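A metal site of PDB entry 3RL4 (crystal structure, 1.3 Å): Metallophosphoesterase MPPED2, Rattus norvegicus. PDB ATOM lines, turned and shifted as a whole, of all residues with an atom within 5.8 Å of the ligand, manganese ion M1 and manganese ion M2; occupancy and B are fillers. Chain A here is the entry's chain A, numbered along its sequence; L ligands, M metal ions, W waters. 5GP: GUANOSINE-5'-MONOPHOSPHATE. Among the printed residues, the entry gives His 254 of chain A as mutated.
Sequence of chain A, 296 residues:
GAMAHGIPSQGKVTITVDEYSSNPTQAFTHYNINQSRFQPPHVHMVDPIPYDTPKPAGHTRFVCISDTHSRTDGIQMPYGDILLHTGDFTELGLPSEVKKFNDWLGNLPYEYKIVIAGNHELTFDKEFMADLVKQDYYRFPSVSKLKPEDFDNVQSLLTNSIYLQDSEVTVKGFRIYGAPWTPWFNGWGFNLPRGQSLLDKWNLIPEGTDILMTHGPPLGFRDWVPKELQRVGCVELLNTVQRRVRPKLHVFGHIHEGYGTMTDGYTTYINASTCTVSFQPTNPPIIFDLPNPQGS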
ATOM      1  N   ASP A  67       3.203  29.815 -17.528  1.00  0.00           N
ATOM      2  CA  ASP A  67       3.126  28.413 -17.113  1.00  0.00           C
ATOM      3  C   ASP A  67       2.051  28.252 -16.048  1.00  0.00           C
ATOM      4  O   ASP A  67       2.251  27.602 -15.012  1.00  0.00           O
ATOM      5  CB  ASP A  67       4.493  27.935 -16.609  1.00  0.00           C
ATOM      6  CG  ASP A  67       5.506  27.926 -17.729  1.00  0.00           C
ATOM      7  OD1 ASP A  67       5.564  26.916 -18.448  1.00  0.00           O
ATOM      8  OD2 ASP A  67       6.197  28.949 -17.915  1.00  0.00           O
ATOM      9  N   HIS A  69      -0.773  26.740 -16.895  1.00  0.00           N
ATOM     10  CA  HIS A  69      -1.151  25.340 -17.157  1.00  0.00           C
ATOM     11  C   HIS A  69      -2.605  25.045 -16.776  1.00  0.00           C
ATOM     12  O   HIS A  69      -2.911  23.967 -16.259  1.00  0.00           O
ATOM     13  CB  HIS A  69      -0.152  24.367 -16.500  1.00  0.00           C
ATOM     14  CG  HIS A  69       1.174  24.286 -17.202  1.00  0.00           C
ATOM     15  ND1 HIS A  69       1.343  23.608 -18.395  1.00  0.00           N
ATOM     16  CD2 HIS A  69       2.384  24.845 -16.923  1.00  0.00           C
ATOM     17  CE1 HIS A  69       2.593  23.709 -18.786  1.00  0.00           C
ATOM     18  NE2 HIS A  69       3.248  24.457 -17.916  1.00  0.00           N
ATOM     19  N   GLY A  87       3.408  32.045 -21.722  1.00  0.00           N
ATOM     20  CA  GLY A  87       3.070  30.801 -22.442  1.00  0.00           C
ATOM     21  C   GLY A  87       2.801  29.628 -21.516  1.00  0.00           C
ATOM     22  O   GLY A  87       2.932  29.710 -20.285  1.00  0.00           O
ATOM     23  N   ASP A  88       2.447  28.490 -22.113  1.00  0.00           N
ATOM     24  CA  ASP A  88       1.954  27.331 -21.340  1.00  0.00           C
ATOM     25  C   ASP A  88       0.758  27.763 -20.475  1.00  0.00           C
ATOM     26  O   ASP A  88       0.707  27.499 -19.253  1.00  0.00           O
ATOM     27  CB  ASP A  88       3.048  26.680 -20.486  1.00  0.00           C
ATOM     28  CG  ASP A  88       3.948  25.728 -21.284  1.00  0.00           C
ATOM     29  OD1 ASP A  88       3.740  25.565 -22.512  1.00  0.00           O
ATOM     30  OD2 ASP A  88       4.889  25.174 -20.637  1.00  0.00           O
ATOM     31  N   GLY A 118       3.320  28.767 -25.411  1.00  0.00           N
ATOM     32  CA  GLY A 118       4.438  27.894 -25.110  1.00  0.00           C
ATOM     33  C   GLY A 118       4.269  26.521 -25.751  1.00  0.00           C
ATOM     34  O   GLY A 118       3.384  26.300 -26.602  1.00  0.00           O
ATOM     35  N   ASN A 119       5.088  25.586 -25.294  1.00  0.00           N
ATOM     36  CA  ASN A 119       5.131  24.268 -25.921  1.00  0.00           C
ATOM     37  C   ASN A 119       3.873  23.437 -25.705  1.00  0.00           C
ATOM     38  O   ASN A 119       3.613  22.482 -26.458  1.00  0.00           O
ATOM     39  CB  ASN A 119       6.409  23.503 -25.536  1.00  0.00           C
ATOM     40  CG  ASN A 119       6.601  23.402 -24.075  1.00  0.00           C
ATOM     41  OD1 ASN A 119       6.678  24.426 -23.381  1.00  0.00           O
ATOM     42  ND2 ASN A 119       6.692  22.198 -23.558  1.00  0.00           N
ATOM     43  N   HIS A 120       3.093  23.759 -24.662  1.00  0.00           N
ATOM     44  CA  HIS A 120       1.835  23.031 -24.456  1.00  0.00           C
ATOM     45  C   HIS A 120       0.693  23.478 -25.341  1.00  0.00           C
ATOM     46  O   HIS A 120      -0.336  22.802 -25.387  1.00  0.00           O
ATOM     47  CB  HIS A 120       1.418  23.068 -22.986  1.00  0.00           C
ATOM     48  CG  HIS A 120       2.237  22.175 -22.123  1.00  0.00           C
ATOM     49  ND1 HIS A 120       1.733  21.004 -21.576  1.00  0.00           N
ATOM     50  CD2 HIS A 120       3.540  22.222 -21.760  1.00  0.00           C
ATOM     51  CE1 HIS A 120       2.673  20.409 -20.866  1.00  0.00           C
ATOM     52  NE2 HIS A 120       3.782  21.122 -20.965  1.00  0.00           N
ATOM     53  N   PRO A 183      14.256  25.433 -27.445  1.00  0.00           N
ATOM     54  CA  PRO A 183      15.087  24.290 -27.834  1.00  0.00           C
ATOM     55  C   PRO A 183      14.328  22.980 -27.726  1.00  0.00           C
ATOM     56  O   PRO A 183      13.657  22.738 -26.712  1.00  0.00           O
ATOM     57  CB  PRO A 183      16.218  24.326 -26.802  1.00  0.00           C
ATOM     58  CG  PRO A 183      16.354  25.774 -26.432  1.00  0.00           C
ATOM     59  CD  PRO A 183      14.931  26.291 -26.440  1.00  0.00           C
ATOM     60  N   TRP A 184      14.481  22.136 -28.737  1.00  0.00           N
ATOM     61  CA  TRP A 184      13.782  20.853 -28.837  1.00  0.00           C
ATOM     62  C   TRP A 184      13.965  20.039 -27.559  1.00  0.00           C
ATOM     63  O   TRP A 184      15.076  19.874 -27.046  1.00  0.00           O
ATOM     64  CB  TRP A 184      14.284  20.075 -30.055  1.00  0.00           C
ATOM     65  CG  TRP A 184      13.293  19.062 -30.657  1.00  0.00           C
ATOM     66  CD1 TRP A 184      12.473  19.267 -31.728  1.00  0.00           C
ATOM     67  CD2 TRP A 184      13.060  17.715 -30.233  1.00  0.00           C
ATOM     68  NE1 TRP A 184      11.732  18.132 -31.993  1.00  0.00           N
ATOM     69  CE2 TRP A 184      12.070  17.170 -31.088  1.00  0.00           C
ATOM     70  CE3 TRP A 184      13.572  16.909 -29.203  1.00  0.00           C
ATOM     71  CZ2 TRP A 184      11.594  15.857 -30.957  1.00  0.00           C
ATOM     72  CZ3 TRP A 184      13.096  15.598 -29.082  1.00  0.00           C
ATOM     73  CH2 TRP A 184      12.121  15.099 -29.948  1.00  0.00           C
ATOM     74  N   PHE A 185      12.850  19.562 -27.046  1.00  0.00           N
ATOM     75  CA  PHE A 185      12.866  18.711 -25.879  1.00  0.00           C
ATOM     76  C   PHE A 185      12.120  17.386 -26.172  1.00  0.00           C
ATOM     77  O   PHE A 185      12.710  16.307 -26.051  1.00  0.00           O
ATOM     78  CB  PHE A 185      12.286  19.488 -24.693  1.00  0.00           C
ATOM     79  CG  PHE A 185      12.223  18.696 -23.423  1.00  0.00           C
ATOM     80  CD1 PHE A 185      13.357  18.088 -22.896  1.00  0.00           C
ATOM     81  CD2 PHE A 185      11.019  18.559 -22.742  1.00  0.00           C
ATOM     82  CE1 PHE A 185      13.294  17.355 -21.707  1.00  0.00           C
ATOM     83  CE2 PHE A 185      10.934  17.833 -21.552  1.00  0.00           C
ATOM     84  CZ  PHE A 185      12.083  17.227 -21.035  1.00  0.00           C
ATOM     85  N   ASN A 186      10.881  17.484 -26.638  1.00  0.00           N
ATOM     86  CA  ASN A 186      10.041  16.281 -26.856  1.00  0.00           C
ATOM     87  C   ASN A 186       9.153  16.388 -28.091  1.00  0.00           C
ATOM     88  O   ASN A 186       8.269  15.570 -28.285  1.00  0.00           O
ATOM     89  CB  ASN A 186       9.170  15.995 -25.630  1.00  0.00           C
ATOM     90  CG  ASN A 186       8.407  17.223 -25.162  1.00  0.00           C
ATOM     91  OD1 ASN A 186       8.279  18.213 -25.906  1.00  0.00           O
ATOM     92  ND2 ASN A 186       7.895  17.180 -23.944  1.00  0.00           N
ATOM     93  N   ARG A 194      18.505  23.295 -31.594  1.00  0.00           N
ATOM     94  CA  ARG A 194      19.450  24.341 -31.273  1.00  0.00           C
ATOM     95  C   ARG A 194      20.257  24.776 -32.491  1.00  0.00           C
ATOM     96  O   ARG A 194      20.458  23.999 -33.437  1.00  0.00           O
ATOM     97  CB  ARG A 194      20.369  23.891 -30.126  1.00  0.00           C
ATOM     98  CG  ARG A 194      19.644  23.766 -28.794  1.00  0.00           C
ATOM     99  CD  ARG A 194      20.535  23.216 -27.658  1.00  0.00           C
ATOM    100  NE  ARG A 194      19.749  22.937 -26.459  1.00  0.00           N
ATOM    101  CZ  ARG A 194      19.434  23.846 -25.529  1.00  0.00           C
ATOM    102  NH1 ARG A 194      19.840  25.111 -25.640  1.00  0.00           N
ATOM    103  NH2 ARG A 194      18.686  23.478 -24.501  1.00  0.00           N
ATOM    104  N   HIS A 215       9.008  31.999 -24.624  1.00  0.00           N
ATOM    105  CA  HIS A 215       8.490  31.032 -23.691  1.00  0.00           C
ATOM    106  C   HIS A 215       9.575  30.543 -22.743  1.00  0.00           C
ATOM    107  O   HIS A 215       9.339  30.355 -21.550  1.00  0.00           O
ATOM    108  CB  HIS A 215       7.783  29.860 -24.350  1.00  0.00           C
ATOM    109  CG  HIS A 215       7.300  28.845 -23.355  1.00  0.00           C
ATOM    110  ND1 HIS A 215       6.498  29.181 -22.279  1.00  0.00           N
ATOM    111  CD2 HIS A 215       7.525  27.506 -23.250  1.00  0.00           C
ATOM    112  CE1 HIS A 215       6.274  28.104 -21.547  1.00  0.00           C
ATOM    113  NE2 HIS A 215       6.888  27.072 -22.100  1.00  0.00           N
ATOM    114  N   VAL A 225      18.153  23.070 -14.740  1.00  0.00           N
ATOM    115  CA  VAL A 225      17.222  21.956 -14.535  1.00  0.00           C
ATOM    116  C   VAL A 225      17.870  20.967 -13.560  1.00  0.00           C
ATOM    117  O   VAL A 225      18.778  20.225 -13.960  1.00  0.00           O
ATOM    118  CB  VAL A 225      16.834  21.248 -15.853  1.00  0.00           C
ATOM    119  CG1 VAL A 225      15.860  20.081 -15.607  1.00  0.00           C
ATOM    120  CG2 VAL A 225      16.206  22.241 -16.816  1.00  0.00           C
ATOM    121  N   GLU A 228      18.390  16.987 -14.443  1.00  0.00           N
ATOM    122  CA  GLU A 228      19.438  16.622 -15.399  1.00  0.00           C
ATOM    123  C   GLU A 228      20.795  17.221 -15.058  1.00  0.00           C
ATOM    124  O   GLU A 228      21.789  16.887 -15.702  1.00  0.00           O
ATOM    125  CB  GLU A 228      19.039  16.995 -16.829  1.00  0.00           C
ATOM    126  CG  GLU A 228      18.070  16.019 -17.504  1.00  0.00           C
ATOM    127  CD  GLU A 228      16.642  16.215 -17.056  1.00  0.00           C
ATOM    128  OE1 GLU A 228      16.311  17.298 -16.530  1.00  0.00           O
ATOM    129  OE2 GLU A 228      15.828  15.278 -17.232  1.00  0.00           O
ATOM    130  N   GLN A 230      21.751  20.251 -15.689  1.00  0.00           N
ATOM    131  CA  GLN A 230      22.140  20.910 -16.930  1.00  0.00           C
ATOM    132  C   GLN A 230      21.485  22.281 -17.034  1.00  0.00           C
ATOM    133  O   GLN A 230      20.367  22.490 -16.569  1.00  0.00           O
ATOM    134  CB  GLN A 230      21.716  20.075 -18.151  1.00  0.00           C
ATOM    135  CG  GLN A 230      22.503  18.794 -18.353  1.00  0.00           C
ATOM    136  CD  GLN A 230      22.278  18.129 -19.701  1.00  0.00           C
ATOM    137  OE1 GLN A 230      21.346  18.478 -20.440  1.00  0.00           O
ATOM    138  NE2 GLN A 230      23.129  17.157 -20.035  1.00  0.00           N
ATOM    139  N   VAL A 232      19.743  24.730 -19.712  1.00  0.00           N
ATOM    140  CA  VAL A 232      18.991  24.394 -20.920  1.00  0.00           C
ATOM    141  C   VAL A 232      18.551  25.633 -21.700  1.00  0.00           C
ATOM    142  O   VAL A 232      17.866  25.488 -22.707  1.00  0.00           O
ATOM    143  CB  VAL A 232      17.768  23.485 -20.637  1.00  0.00           C
ATOM    144  CG1 VAL A 232      18.195  22.182 -19.901  1.00  0.00           C
ATOM    145  CG2 VAL A 232      16.720  24.238 -19.819  1.00  0.00           C
ATOM    146  N   HIS A 254       8.892  28.504 -18.803  1.00  0.00           N
ATOM    147  CA  HIS A 254       9.253  27.181 -19.356  1.00  0.00           C
ATOM    148  C   HIS A 254       9.972  26.279 -18.373  1.00  0.00           C
ATOM    149  O   HIS A 254       9.579  25.117 -18.200  1.00  0.00           O
ATOM    150  CB  HIS A 254      10.006  27.334 -20.682  1.00  0.00           C
ATOM    151  CG  HIS A 254      10.256  26.044 -21.403  1.00  0.00           C
ATOM    152  ND1 HIS A 254       9.261  25.129 -21.699  1.00  0.00           N
ATOM    153  CD2 HIS A 254      11.404  25.540 -21.905  1.00  0.00           C
ATOM    154  CE1 HIS A 254       9.784  24.131 -22.389  1.00  0.00           C
ATOM    155  NE2 HIS A 254      11.086  24.355 -22.522  1.00  0.00           N
ATOM    156  N   ILE A 255      11.064  26.797 -17.817  1.00  0.00           N
ATOM    157  CA  ILE A 255      11.789  26.064 -16.781  1.00  0.00           C
ATOM    158  C   ILE A 255      11.223  26.479 -15.442  1.00  0.00           C
ATOM    159  O   ILE A 255      11.634  27.507 -14.866  1.00  0.00           O
ATOM    160  CB  ILE A 255      13.310  26.293 -16.898  1.00  0.00           C
ATOM    161  CG1 ILE A 255      13.805  25.937 -18.318  1.00  0.00           C
ATOM    162  CG2 ILE A 255      14.061  25.519 -15.798  1.00  0.00           C
ATOM    163  CD1 ILE A 255      13.374  24.561 -18.851  1.00  0.00           C
ATOM    164  N   HIS A 256      10.237  25.711 -14.985  1.00  0.00           N
ATOM    165  CA  HIS A 256       9.441  26.137 -13.820  1.00  0.00           C
ATOM    166  C   HIS A 256      10.313  26.378 -12.599  1.00  0.00           C
ATOM    167  O   HIS A 256      10.078  27.326 -11.823  1.00  0.00           O
ATOM    168  CB  HIS A 256       8.380  25.086 -13.502  1.00  0.00           C
ATOM    169  CG  HIS A 256       7.343  24.878 -14.566  1.00  0.00           C
ATOM    170  ND1 HIS A 256       6.298  23.996 -14.378  1.00  0.00           N
ATOM    171  CD2 HIS A 256       7.189  25.385 -15.824  1.00  0.00           C
ATOM    172  CE1 HIS A 256       5.535  23.975 -15.463  1.00  0.00           C
ATOM    173  NE2 HIS A 256       6.053  24.803 -16.352  1.00  0.00           N
ATOM    174  N   GLU A 257      11.341  25.543 -12.455  1.00  0.00           N
ATOM    175  CA  GLU A 257      12.279  25.551 -11.329  1.00  0.00           C
ATOM    176  C   GLU A 257      13.035  26.866 -11.243  1.00  0.00           C
ATOM    177  O   GLU A 257      13.563  27.216 -10.187  1.00  0.00           O
ATOM    178  CB  GLU A 257      13.312  24.423 -11.457  1.00  0.00           C
ATOM    179  CG  GLU A 257      12.784  22.994 -11.615  1.00  0.00           C
ATOM    180  CD  GLU A 257      12.658  22.611 -13.069  1.00  0.00           C
ATOM    181  OE1 GLU A 257      11.865  23.241 -13.770  1.00  0.00           O
ATOM    182  OE2 GLU A 257      13.305  21.638 -13.518  1.00  0.00           O
ATOM    183  N   THR A 276       5.164  25.300 -10.189  1.00  0.00           N
ATOM    184  CA  THR A 276       6.428  24.656  -9.841  1.00  0.00           C
ATOM    185  C   THR A 276       6.674  23.464 -10.798  1.00  0.00           C
ATOM    186  O   THR A 276       5.846  23.146 -11.667  1.00  0.00           O
ATOM    187  CB  THR A 276       6.333  24.094  -8.424  1.00  0.00           C
ATOM    188  OG1 THR A 276       5.291  23.117  -8.407  1.00  0.00           O
ATOM    189  CG2 THR A 276       6.051  25.211  -7.412  1.00  0.00           C
ATOM    190  N   VAL A 277       7.813  22.801 -10.649  1.00  0.00           N
ATOM    191  CA  VAL A 277       8.106  21.632 -11.468  1.00  0.00           C
ATOM    192  C   VAL A 277       7.063  20.497 -11.309  1.00  0.00           C
ATOM    193  O   VAL A 277       6.903  19.656 -12.201  1.00  0.00           O
ATOM    194  CB  VAL A 277       9.563  21.141 -11.260  1.00  0.00           C
ATOM    195  CG1 VAL A 277       9.737  20.530  -9.880  1.00  0.00           C
ATOM    196  CG2 VAL A 277      10.008  20.172 -12.394  1.00  0.00           C
ATOM    197  N   PHE A 279       3.902  21.221 -11.085  1.00  0.00           N
ATOM    198  CA  PHE A 279       2.684  21.797 -11.670  1.00  0.00           C
ATOM    199  C   PHE A 279       1.698  22.352 -10.615  1.00  0.00           C
ATOM    200  O   PHE A 279       0.477  22.348 -10.826  1.00  0.00           O
ATOM    201  CB  PHE A 279       2.017  20.814 -12.669  1.00  0.00           C
ATOM    202  CG  PHE A 279       2.702  20.741 -14.020  1.00  0.00           C
ATOM    203  CD1 PHE A 279       3.958  20.137 -14.164  1.00  0.00           C
ATOM    204  CD2 PHE A 279       2.100  21.271 -15.157  1.00  0.00           C
ATOM    205  CE1 PHE A 279       4.585  20.074 -15.422  1.00  0.00           C
ATOM    206  CE2 PHE A 279       2.719  21.199 -16.407  1.00  0.00           C
ATOM    207  CZ  PHE A 279       3.954  20.614 -16.537  1.00  0.00           C
HETATM  208  P   5GP L   1       6.737  22.136 -19.746  1.00  0.00           P
HETATM  209  O1P 5GP L   1       7.090  22.845 -20.987  1.00  0.00           O
HETATM  210  O2P 5GP L   1       5.540  22.816 -18.893  1.00  0.00           O
HETATM  211  O3P 5GP L   1       6.232  20.689 -20.070  1.00  0.00           O
HETATM  212  O5' 5GP L   1       8.018  22.022 -18.793  1.00  0.00           O
HETATM  213  C5' 5GP L   1       7.932  21.363 -17.508  1.00  0.00           C
HETATM  214  C4' 5GP L   1       9.312  21.011 -16.988  1.00  0.00           C
HETATM  215  O4' 5GP L   1       9.946  20.197 -17.987  1.00  0.00           O
HETATM  216  C3' 5GP L   1      10.295  22.171 -16.837  1.00  0.00           C
HETATM  217  O3' 5GP L   1      10.040  22.900 -15.616  1.00  0.00           O
HETATM  218  C2' 5GP L   1      11.620  21.420 -16.815  1.00  0.00           C
HETATM  219  O2' 5GP L   1      11.818  20.754 -15.558  1.00  0.00           O
HETATM  220  C1' 5GP L   1      11.365  20.340 -17.889  1.00  0.00           C
HETATM  221  N9  5GP L   1      11.912  20.812 -19.195  1.00  0.00           N
HETATM  222  C8  5GP L   1      11.348  21.642 -20.099  1.00  0.00           C
HETATM  223  N7  5GP L   1      12.182  21.807 -21.115  1.00  0.00           N
HETATM  224  C5  5GP L   1      13.285  21.104 -20.873  1.00  0.00           C
HETATM  225  C6  5GP L   1      14.477  20.910 -21.558  1.00  0.00           C
HETATM  226  O6  5GP L   1      14.716  21.432 -22.655  1.00  0.00           O
HETATM  227  N1  5GP L   1      15.427  20.078 -20.997  1.00  0.00           N
HETATM  228  C2  5GP L   1      15.201  19.470 -19.754  1.00  0.00           C
HETATM  229  N2  5GP L   1      16.138  18.677 -19.246  1.00  0.00           N
HETATM  230  N3  5GP L   1      14.045  19.665 -19.109  1.00  0.00           N
HETATM  231  C4  5GP L   1      13.101  20.470 -19.645  1.00  0.00           C
HETATM  232 MN    MN M   1       7.015  24.982 -21.371  1.00  0.00          MN
HETATM  233 MN    MN M   2       5.305  24.867 -18.449  1.00  0.00          MN
HETATM  234  O   HOH W   1      12.583  18.244 -14.791  1.00  0.00           O
HETATM  235  O   HOH W   2      17.585  18.743 -22.109  1.00  0.00           O
HETATM  236  O   HOH W   3      13.718  23.713 -23.878  1.00  0.00           O
HETATM  237  O   HOH W   4       7.129  24.977 -19.443  1.00  0.00           O
HETATM  238  O   HOH W   5      16.711  20.935 -24.511  1.00  0.00           O
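Residues that only touch the ligand: Phe 185, Phe 279, Val 232, Val 277, Ile 255 and Val 225.
Hydrophobic or aromatic side chains within 4 Å of the ligand: His 69, His 120, Phe 185, Val 225, Val 232, His 254, Ile 255, His 256, Val 277 and Phe 279.
Within 4 Å of the ligand: His 69, Asp 88, Asn 119, His 120, Phe 185, Val 225, Glu 228, Val 232, His 254, Ile 255, His 256, Glu 257, Val 277 and Phe 279.
The nearest printed residue that does not touch the ligand is Asp 67 (4.1 Å).
Water W4 bridges the backbone carbonyl oxygen (O) of His 254 and an oxygen (O5') of the ligand.
Water W5 lies within hydrogen-bond range of an oxygen (O6) of the ligand (2.8 Å), the backbone carbonyl oxygen (O) of Trp 184 (3.2 Å) and the guanidinium group (NH2) of Arg 194 (3.2 Å).
Water W3 lies within hydrogen-bond range of O6 of the ligand (2.8 Å), O of Pro 183 (3.0 Å) and NE2 of His 254 (3.0 Å).
Four residues have an atom within 4 Å of manganese ion M2: Asp 67, His 69, Asp 88 and His 256.
The nearest printed residue that does not touch manganese ion M2 is His 254 (4.3 Å).
The backbone NH (N) of His 254 sits at hydrogen-bond distance from the side-chain carboxylate (OD2) of Asp 67.
N of Asp 67 sits at hydrogen-bond distance from O of Gly 87, at 2.8 Å.
A ring nitrogen (ND1) of His 256 is in hydrogen-bond range of the backbone carbonyl oxygen (O) of Thr 276, 2.9 Å away.
The backbone NH of His 120 is in hydrogen-bond range of the side-chain carboxylate of Asp 88, at 2.9 Å.
O of Val 232 lies within hydrogen-bond range of NH2 of Arg 194 (2.8 Å).
The backbone NH (N) of Val 225 is in hydrogen-bond range of the backbone carbonyl oxygen (O) of Gln 230, 2.9 Å away.
Manganese ion M1 is bound by water W4 (1.9 Å), OD1 of Asn 119 (2.1 Å), O1P of the ligand (2.2 Å), NE2 of His 215 (2.2 Å), OD2 of Asp 88 (2.3 Å) and ND1 of His 254 (2.3 Å).
N of His 256 sits at hydrogen-bond distance from O3' of the ligand.
An oxygen (O3') of the ligand lies close to the backbone carbonyl oxygen (O) of His 254, 3.4 Å away.
The side-chain carboxylate (OE1) of Glu 257 is in hydrogen-bond range of an oxygen (O3') of the ligand, at 2.6 Å.
A ring nitrogen (NE2) of His 120 is in hydrogen-bond range of an oxygen (O3P) of the ligand (2.6 Å).
The side-chain carboxylate (OE1) of Glu 228 sits at hydrogen-bond distance from a nitrogen (N2) of the ligand (3.1 Å).
Of the 24 residues printed, 5 come within 4 Å of manganese ion M1.
The nearest printed residue that does not touch manganese ion M1 is His 120 (4.5 Å).
Manganese ion M2 is bound by the side-chain carboxylate (OD1) of Asp 67, at 2.1 Å.
Water W4 binds manganese ion M2, 2.1 Å away.
An oxygen (O2P) of the ligand binds manganese ion M2 (2.1 Å).
Manganese ion M2 is bound by a ring nitrogen (NE2) of His 69, at 2.2 Å.
NE2 of His 256 is bound to manganese ion M2, 2.2 Å away.
The side-chain carboxylate (OD2) of Asp 88 binds manganese ion M2, at 2.2 Å.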
